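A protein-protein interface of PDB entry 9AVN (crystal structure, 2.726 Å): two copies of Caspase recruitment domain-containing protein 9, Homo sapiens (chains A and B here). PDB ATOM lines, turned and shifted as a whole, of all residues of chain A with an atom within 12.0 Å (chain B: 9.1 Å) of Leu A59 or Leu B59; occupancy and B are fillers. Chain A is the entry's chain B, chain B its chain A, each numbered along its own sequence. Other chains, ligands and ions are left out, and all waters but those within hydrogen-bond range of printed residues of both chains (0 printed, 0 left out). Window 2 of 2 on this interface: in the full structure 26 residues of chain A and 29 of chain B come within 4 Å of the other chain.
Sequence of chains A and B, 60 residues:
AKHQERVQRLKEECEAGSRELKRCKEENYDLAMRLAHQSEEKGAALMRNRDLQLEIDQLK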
ATOM      1  N   ARG A  50      13.399 -10.613 -15.381  1.00  0.00           N
ATOM      2  CA  ARG A  50      12.874  -9.500 -16.152  1.00  0.00           C
ATOM      3  C   ARG A  50      14.012  -8.722 -16.794  1.00  0.00           C
ATOM      4  O   ARG A  50      13.976  -8.481 -17.999  1.00  0.00           O
ATOM      5  CB  ARG A  50      12.021  -8.612 -15.245  1.00  0.00           C
ATOM      6  CG  ARG A  50      11.544  -7.309 -15.872  1.00  0.00           C
ATOM      7  CD  ARG A  50      10.878  -6.421 -14.823  1.00  0.00           C
ATOM      8  NE  ARG A  50      11.788  -6.086 -13.719  1.00  0.00           N
ATOM      9  CZ  ARG A  50      11.581  -6.414 -12.445  1.00  0.00           C
ATOM     10  NH1 ARG A  50      12.469  -6.079 -11.514  1.00  0.00           N
ATOM     11  NH2 ARG A  50      10.489  -7.086 -12.093  1.00  0.00           N
ATOM     12  N   ASP A  51      15.052  -8.400 -16.006  1.00  0.00           N
ATOM     13  CA  ASP A  51      16.217  -7.651 -16.469  1.00  0.00           C
ATOM     14  C   ASP A  51      17.081  -8.461 -17.441  1.00  0.00           C
ATOM     15  O   ASP A  51      17.671  -7.889 -18.359  1.00  0.00           O
ATOM     16  CB  ASP A  51      17.038  -7.136 -15.272  1.00  0.00           C
ATOM     17  CG  ASP A  51      16.288  -6.128 -14.407  1.00  0.00           C
ATOM     18  OD1 ASP A  51      15.487  -5.347 -14.967  1.00  0.00           O
ATOM     19  OD2 ASP A  51      16.513  -6.113 -13.170  1.00  0.00           O
ATOM     20  N   LEU A  52      17.126  -9.794 -17.266  1.00  0.00           N
ATOM     21  CA  LEU A  52      17.876 -10.675 -18.160  1.00  0.00           C
ATOM     22  C   LEU A  52      17.193 -10.761 -19.518  1.00  0.00           C
ATOM     23  O   LEU A  52      17.869 -10.780 -20.539  1.00  0.00           O
ATOM     24  CB  LEU A  52      17.983 -12.080 -17.563  1.00  0.00           C
ATOM     25  CG  LEU A  52      19.166 -12.361 -16.656  1.00  0.00           C
ATOM     26  CD1 LEU A  52      19.133 -13.787 -16.181  1.00  0.00           C
ATOM     27  CD2 LEU A  52      20.488 -12.080 -17.357  1.00  0.00           C
ATOM     28  N   GLN A  53      15.852 -10.832 -19.523  1.00  0.00           N
ATOM     29  CA  GLN A  53      15.007 -10.877 -20.717  1.00  0.00           C
ATOM     30  C   GLN A  53      15.149  -9.572 -21.513  1.00  0.00           C
ATOM     31  O   GLN A  53      15.148  -9.605 -22.740  1.00  0.00           O
ATOM     32  CB  GLN A  53      13.545 -11.101 -20.307  1.00  0.00           C
ATOM     33  CG  GLN A  53      12.595 -11.326 -21.459  1.00  0.00           C
ATOM     34  CD  GLN A  53      12.968 -12.531 -22.277  1.00  0.00           C
ATOM     35  OE1 GLN A  53      12.932 -13.671 -21.803  1.00  0.00           O
ATOM     36  NE2 GLN A  53      13.333 -12.304 -23.531  1.00  0.00           N
ATOM     37  N   LEU A  54      15.322  -8.431 -20.814  1.00  0.00           N
ATOM     38  CA  LEU A  54      15.537  -7.128 -21.429  1.00  0.00           C
ATOM     39  C   LEU A  54      16.839  -7.142 -22.223  1.00  0.00           C
ATOM     40  O   LEU A  54      16.880  -6.696 -23.365  1.00  0.00           O
ATOM     41  CB  LEU A  54      15.635  -6.055 -20.341  1.00  0.00           C
ATOM     42  CG  LEU A  54      14.520  -5.044 -20.294  1.00  0.00           C
ATOM     43  CD1 LEU A  54      14.398  -4.279 -21.614  1.00  0.00           C
ATOM     44  CD2 LEU A  54      13.215  -5.693 -19.884  1.00  0.00           C
ATOM     45  N   GLU A  55      17.890  -7.693 -21.625  1.00  0.00           N
ATOM     46  CA  GLU A  55      19.211  -7.795 -22.218  1.00  0.00           C
ATOM     47  C   GLU A  55      19.182  -8.654 -23.490  1.00  0.00           C
ATOM     48  O   GLU A  55      19.904  -8.361 -24.442  1.00  0.00           O
ATOM     49  CB  GLU A  55      20.156  -8.386 -21.171  1.00  0.00           C
ATOM     50  CG  GLU A  55      21.631  -8.131 -21.389  1.00  0.00           C
ATOM     51  CD  GLU A  55      22.521  -8.748 -20.319  1.00  0.00           C
ATOM     52  OE1 GLU A  55      23.751  -8.813 -20.550  1.00  0.00           O
ATOM     53  OE2 GLU A  55      21.999  -9.163 -19.256  1.00  0.00           O
ATOM     54  N   ILE A  56      18.347  -9.713 -23.500  1.00  0.00           N
ATOM     55  CA  ILE A  56      18.179 -10.604 -24.652  1.00  0.00           C
ATOM     56  C   ILE A  56      17.467  -9.852 -25.784  1.00  0.00           C
ATOM     57  O   ILE A  56      17.864  -9.970 -26.942  1.00  0.00           O
ATOM     58  CB  ILE A  56      17.439 -11.919 -24.226  1.00  0.00           C
ATOM     59  CG1 ILE A  56      18.435 -12.995 -23.775  1.00  0.00           C
ATOM     60  CG2 ILE A  56      16.491 -12.486 -25.308  1.00  0.00           C
ATOM     61  CD1 ILE A  56      19.247 -13.713 -24.907  1.00  0.00           C
ATOM     62  N   ASP A  57      16.429  -9.072 -25.437  1.00  0.00           N
ATOM     63  CA  ASP A  57      15.638  -8.312 -26.399  1.00  0.00           C
ATOM     64  C   ASP A  57      16.472  -7.274 -27.160  1.00  0.00           C
ATOM     65  O   ASP A  57      16.204  -7.008 -28.333  1.00  0.00           O
ATOM     66  CB  ASP A  57      14.421  -7.671 -25.707  1.00  0.00           C
ATOM     67  CG  ASP A  57      13.388  -8.677 -25.217  1.00  0.00           C
ATOM     68  OD1 ASP A  57      12.563  -8.309 -24.349  1.00  0.00           O
ATOM     69  OD2 ASP A  57      13.418  -9.842 -25.686  1.00  0.00           O
ATOM     70  N   GLN A  58      17.508  -6.725 -26.506  1.00  0.00           N
ATOM     71  CA  GLN A  58      18.404  -5.742 -27.109  1.00  0.00           C
ATOM     72  C   GLN A  58      19.424  -6.369 -28.064  1.00  0.00           C
ATOM     73  O   GLN A  58      19.930  -5.681 -28.952  1.00  0.00           O
ATOM     74  CB  GLN A  58      19.102  -4.920 -26.026  1.00  0.00           C
ATOM     75  CG  GLN A  58      18.117  -4.063 -25.240  1.00  0.00           C
ATOM     76  CD  GLN A  58      18.627  -3.558 -23.906  1.00  0.00           C
ATOM     77  OE1 GLN A  58      18.133  -2.546 -23.382  1.00  0.00           O
ATOM     78  NE2 GLN A  58      19.601  -4.257 -23.307  1.00  0.00           N
ATOM     79  N   LEU A  59      19.725  -7.667 -27.896  1.00  0.00           N
ATOM     80  CA  LEU A  59      20.661  -8.377 -28.771  1.00  0.00           C
ATOM     81  C   LEU A  59      19.878  -9.249 -29.773  1.00  0.00           C
ATOM     82  O   LEU A  59      20.280 -10.377 -30.063  1.00  0.00           O
ATOM     83  CB  LEU A  59      21.619  -9.253 -27.941  1.00  0.00           C
ATOM     84  CG  LEU A  59      22.272  -8.595 -26.716  1.00  0.00           C
ATOM     85  CD1 LEU A  59      23.123  -9.584 -25.955  1.00  0.00           C
ATOM     86  CD2 LEU A  59      23.095  -7.388 -27.113  1.00  0.00           C
ATOM     87  N   LYS A  60      18.742  -8.733 -30.271  1.00  0.00           N
ATOM     88  CA  LYS A  60      17.883  -9.451 -31.209  1.00  0.00           C
ATOM     89  C   LYS A  60      17.886  -8.784 -32.593  1.00  0.00           C
ATOM     90  O   LYS A  60      17.297  -7.718 -32.769  1.00  0.00           O
ATOM     91  CB  LYS A  60      16.447  -9.538 -30.658  1.00  0.00           C
ATOM     92  CG  LYS A  60      16.199 -10.744 -29.766  1.00  0.00           C
ATOM     93  CD  LYS A  60      15.065 -10.469 -28.782  1.00  0.00           C
ATOM     94  CE  LYS A  60      14.223 -11.684 -28.483  1.00  0.00           C
ATOM     95  NZ  LYS A  60      15.033 -12.925 -28.397  1.00  0.00           N
ATOM     96  N   LEU B  52      18.746 -18.305 -19.596  1.00  0.00           N
ATOM     97  CA  LEU B  52      18.825 -16.941 -20.094  1.00  0.00           C
ATOM     98  C   LEU B  52      20.229 -16.417 -20.083  1.00  0.00           C
ATOM     99  O   LEU B  52      20.661 -15.831 -21.070  1.00  0.00           O
ATOM    100  CB  LEU B  52      17.882 -15.988 -19.338  1.00  0.00           C
ATOM    101  CG  LEU B  52      16.530 -15.713 -20.036  1.00  0.00           C
ATOM    102  CD1 LEU B  52      15.693 -14.684 -19.261  1.00  0.00           C
ATOM    103  CD2 LEU B  52      16.717 -15.259 -21.495  1.00  0.00           C
ATOM    104  N   GLN B  53      20.963 -16.678 -18.997  1.00  0.00           N
ATOM    105  CA  GLN B  53      22.340 -16.226 -18.901  1.00  0.00           C
ATOM    106  C   GLN B  53      23.261 -16.840 -19.968  1.00  0.00           C
ATOM    107  O   GLN B  53      23.953 -16.105 -20.666  1.00  0.00           O
ATOM    108  CB  GLN B  53      22.909 -16.459 -17.504  1.00  0.00           C
ATOM    109  CG  GLN B  53      24.237 -15.779 -17.317  1.00  0.00           C
ATOM    110  CD  GLN B  53      24.066 -14.290 -17.313  1.00  0.00           C
ATOM    111  OE1 GLN B  53      23.463 -13.735 -16.396  1.00  0.00           O
ATOM    112  NE2 GLN B  53      24.577 -13.616 -18.341  1.00  0.00           N
ATOM    113  N   LEU B  54      23.215 -18.171 -20.141  1.00  0.00           N
ATOM    114  CA  LEU B  54      24.022 -18.894 -21.109  1.00  0.00           C
ATOM    115  C   LEU B  54      23.800 -18.364 -22.521  1.00  0.00           C
ATOM    116  O   LEU B  54      24.758 -18.176 -23.263  1.00  0.00           O
ATOM    117  CB  LEU B  54      23.659 -20.379 -21.032  1.00  0.00           C
ATOM    118  CG  LEU B  54      24.747 -21.364 -21.428  1.00  0.00           C
ATOM    119  CD1 LEU B  54      26.030 -21.166 -20.609  1.00  0.00           C
ATOM    120  CD2 LEU B  54      24.238 -22.789 -21.330  1.00  0.00           C
ATOM    121  N   GLU B  55      22.550 -18.075 -22.872  1.00  0.00           N
ATOM    122  CA  GLU B  55      22.153 -17.556 -24.174  1.00  0.00           C
ATOM    123  C   GLU B  55      22.720 -16.137 -24.387  1.00  0.00           C
ATOM    124  O   GLU B  55      23.089 -15.789 -25.507  1.00  0.00           O
ATOM    125  CB  GLU B  55      20.624 -17.554 -24.234  1.00  0.00           C
ATOM    126  CG  GLU B  55      20.019 -17.534 -25.616  1.00  0.00           C
ATOM    127  CD  GLU B  55      18.491 -17.525 -25.599  1.00  0.00           C
ATOM    128  OE1 GLU B  55      17.894 -17.079 -26.610  1.00  0.00           O
ATOM    129  OE2 GLU B  55      17.891 -17.956 -24.583  1.00  0.00           O
ATOM    130  N   ILE B  56      22.777 -15.325 -23.323  1.00  0.00           N
ATOM    131  CA  ILE B  56      23.324 -13.968 -23.350  1.00  0.00           C
ATOM    132  C   ILE B  56      24.843 -14.031 -23.554  1.00  0.00           C
ATOM    133  O   ILE B  56      25.388 -13.259 -24.340  1.00  0.00           O
ATOM    134  CB  ILE B  56      22.928 -13.202 -22.050  1.00  0.00           C
ATOM    135  CG1 ILE B  56      21.548 -12.551 -22.168  1.00  0.00           C
ATOM    136  CG2 ILE B  56      23.993 -12.181 -21.583  1.00  0.00           C
ATOM    137  CD1 ILE B  56      21.522 -11.324 -23.108  1.00  0.00           C
ATOM    138  N   ASP B  57      25.510 -14.960 -22.856  1.00  0.00           N
ATOM    139  CA  ASP B  57      26.956 -15.123 -22.925  1.00  0.00           C
ATOM    140  C   ASP B  57      27.440 -15.489 -24.325  1.00  0.00           C
ATOM    141  O   ASP B  57      28.537 -15.098 -24.723  1.00  0.00           O
ATOM    142  CB  ASP B  57      27.436 -16.146 -21.878  1.00  0.00           C
ATOM    143  CG  ASP B  57      27.310 -15.673 -20.435  1.00  0.00           C
ATOM    144  OD1 ASP B  57      27.357 -16.534 -19.520  1.00  0.00           O
ATOM    145  OD2 ASP B  57      27.148 -14.440 -20.219  1.00  0.00           O
ATOM    146  N   GLN B  58      26.614 -16.216 -25.079  1.00  0.00           N
ATOM    147  CA  GLN B  58      26.942 -16.621 -26.447  1.00  0.00           C
ATOM    148  C   GLN B  58      26.766 -15.486 -27.458  1.00  0.00           C
ATOM    149  O   GLN B  58      27.372 -15.528 -28.518  1.00  0.00           O
ATOM    150  CB  GLN B  58      26.119 -17.844 -26.854  1.00  0.00           C
ATOM    151  CG  GLN B  58      26.451 -19.083 -26.033  1.00  0.00           C
ATOM    152  CD  GLN B  58      25.396 -20.169 -26.123  1.00  0.00           C
ATOM    153  OE1 GLN B  58      25.698 -21.355 -25.955  1.00  0.00           O
ATOM    154  NE2 GLN B  58      24.126 -19.801 -26.366  1.00  0.00           N
ATOM    155  N   LEU B  59      25.948 -14.480 -27.140  1.00  0.00           N
ATOM    156  CA  LEU B  59      25.739 -13.346 -28.035  1.00  0.00           C
ATOM    157  C   LEU B  59      26.541 -12.136 -27.530  1.00  0.00           C
ATOM    158  O   LEU B  59      26.063 -11.007 -27.607  1.00  0.00           O
ATOM    159  CB  LEU B  59      24.231 -13.004 -28.128  1.00  0.00           C
ATOM    160  CG  LEU B  59      23.270 -14.183 -28.369  1.00  0.00           C
ATOM    161  CD1 LEU B  59      21.833 -13.722 -28.357  1.00  0.00           C
ATOM    162  CD2 LEU B  59      23.577 -14.882 -29.667  1.00  0.00           C
ATOM    163  N   LYS B  60      27.751 -12.375 -26.993  1.00  0.00           N
ATOM    164  CA  LYS B  60      28.619 -11.329 -26.436  1.00  0.00           C
ATOM    165  C   LYS B  60      29.876 -11.127 -27.284  1.00  0.00           C
ATOM    166  O   LYS B  60      30.759 -11.979 -27.276  1.00  0.00           O
ATOM    167  CB  LYS B  60      29.013 -11.667 -24.985  1.00  0.00           C
ATOM    168  CG  LYS B  60      28.028 -11.167 -23.946  1.00  0.00           C
ATOM    169  CD  LYS B  60      28.070 -12.028 -22.697  1.00  0.00           C
ATOM    170  CE  LYS B  60      27.812 -11.257 -21.419  1.00  0.00           C
ATOM    171  NZ  LYS B  60      26.797 -10.189 -21.592  1.00  0.00           N
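The side-chain amino group (NZ) of Lys B60 is in salt-bridge range of the side-chain carboxylate (OE1) of Glu A55 (3.5 Å).
The side-chain amide nitrogen of Gln A53 is in hydrogen-bond range of the side-chain carboxylate of Asp A57 (3.3 Å).
The side-chain amide nitrogen (NE2) of Gln B53 lies within hydrogen-bond range of the side-chain carboxylate (OD2) of Asp B57, at 3.3 Å.
Leu A52 touches Leu B52.
OE1 of Gln B53 touches CD2 of Leu A52, 3.5 Å away.
Leu B52 touches Gln A53 (CD1 to N, 3.9 Å).
OE1 of Glu A55 touches CG2 of Ile B56 (3.5 Å).
Ile A56 touches Leu B52.
Ile A56 touches Glu B55 (CD1 to CD, 3.9 Å).
Ile A56 touches Ile B56.
CD1 of Leu A59 touches CD1 of Ile B56 (3.7 Å).
Leu A59 touches Leu B59 (CD1 to O, 3.7 Å).
Printed residues of chain B within 4 Å of Leu A59: Ile B56 (3.7 Å) and Leu B59 (3.7 Å).
Of chain A, only Leu A59 comes within 4 Å of Leu B59.
Glu B55 touches just one residue of chain A: Ile A56 (3.9 Å).
Ile B56 touches three residues of chain A.
No residue of chain A comes within 4 Å of Gln B58.
Of the printed residues of chain B, Glu A55 touches Ile B56 (3.5 Å) and Lys B60 (3.5 Å).
Of the printed residues of chain B, Ile A56 touches Leu B52, Glu B55 and Ile B56.
Of the printed residues of chain A, Leu B52 touches Leu A52 (3.9 Å), Gln A53 (3.9 Å) and Ile A56 (3.6 Å).
Of the printed residues of chain A, Gln B53 touches Leu A52 (3.5 Å).
Printed residues of chain B within 4 Å of Leu A52: Leu B52 and Gln B53.
The nearest residue of chain B that does not touch Leu A59 is Lys B60 (5.5 Å).
The nearest printed residue of chain B that does not touch Leu A52 is Ile B56 (4.4 Å).
Hydrophobic or aromatic side chains of chain B within 4 Å of the printed part of chain A: Leu B52 and Ile B56.
Along chain B the printed residues that touch a printed residue of chain A span positions 52 to 60.
Among the printed residues, Asp or Glu carboxylates within 4 Å of a Lys or Arg side-chain nitrogen of the other chain: Glu A55 with Lys B60.
Ile A56 touches Leu B52, but with the chains exchanged Leu A52 does not touch Ile B56 (4.4 Å).
Ile A56 touches its own counterpart, Ile B56.
Leu A59 touches Ile B56, but with the chains exchanged Ile A56 does not touch Leu B59 (4.3 Å).
Leu A59 touches its own counterpart, Leu B59.
9 positions are printed for both chains.
Of the 10 pairs that touch across the chains among the printed residues, 7 have their exchanged pair printed and touching as well.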
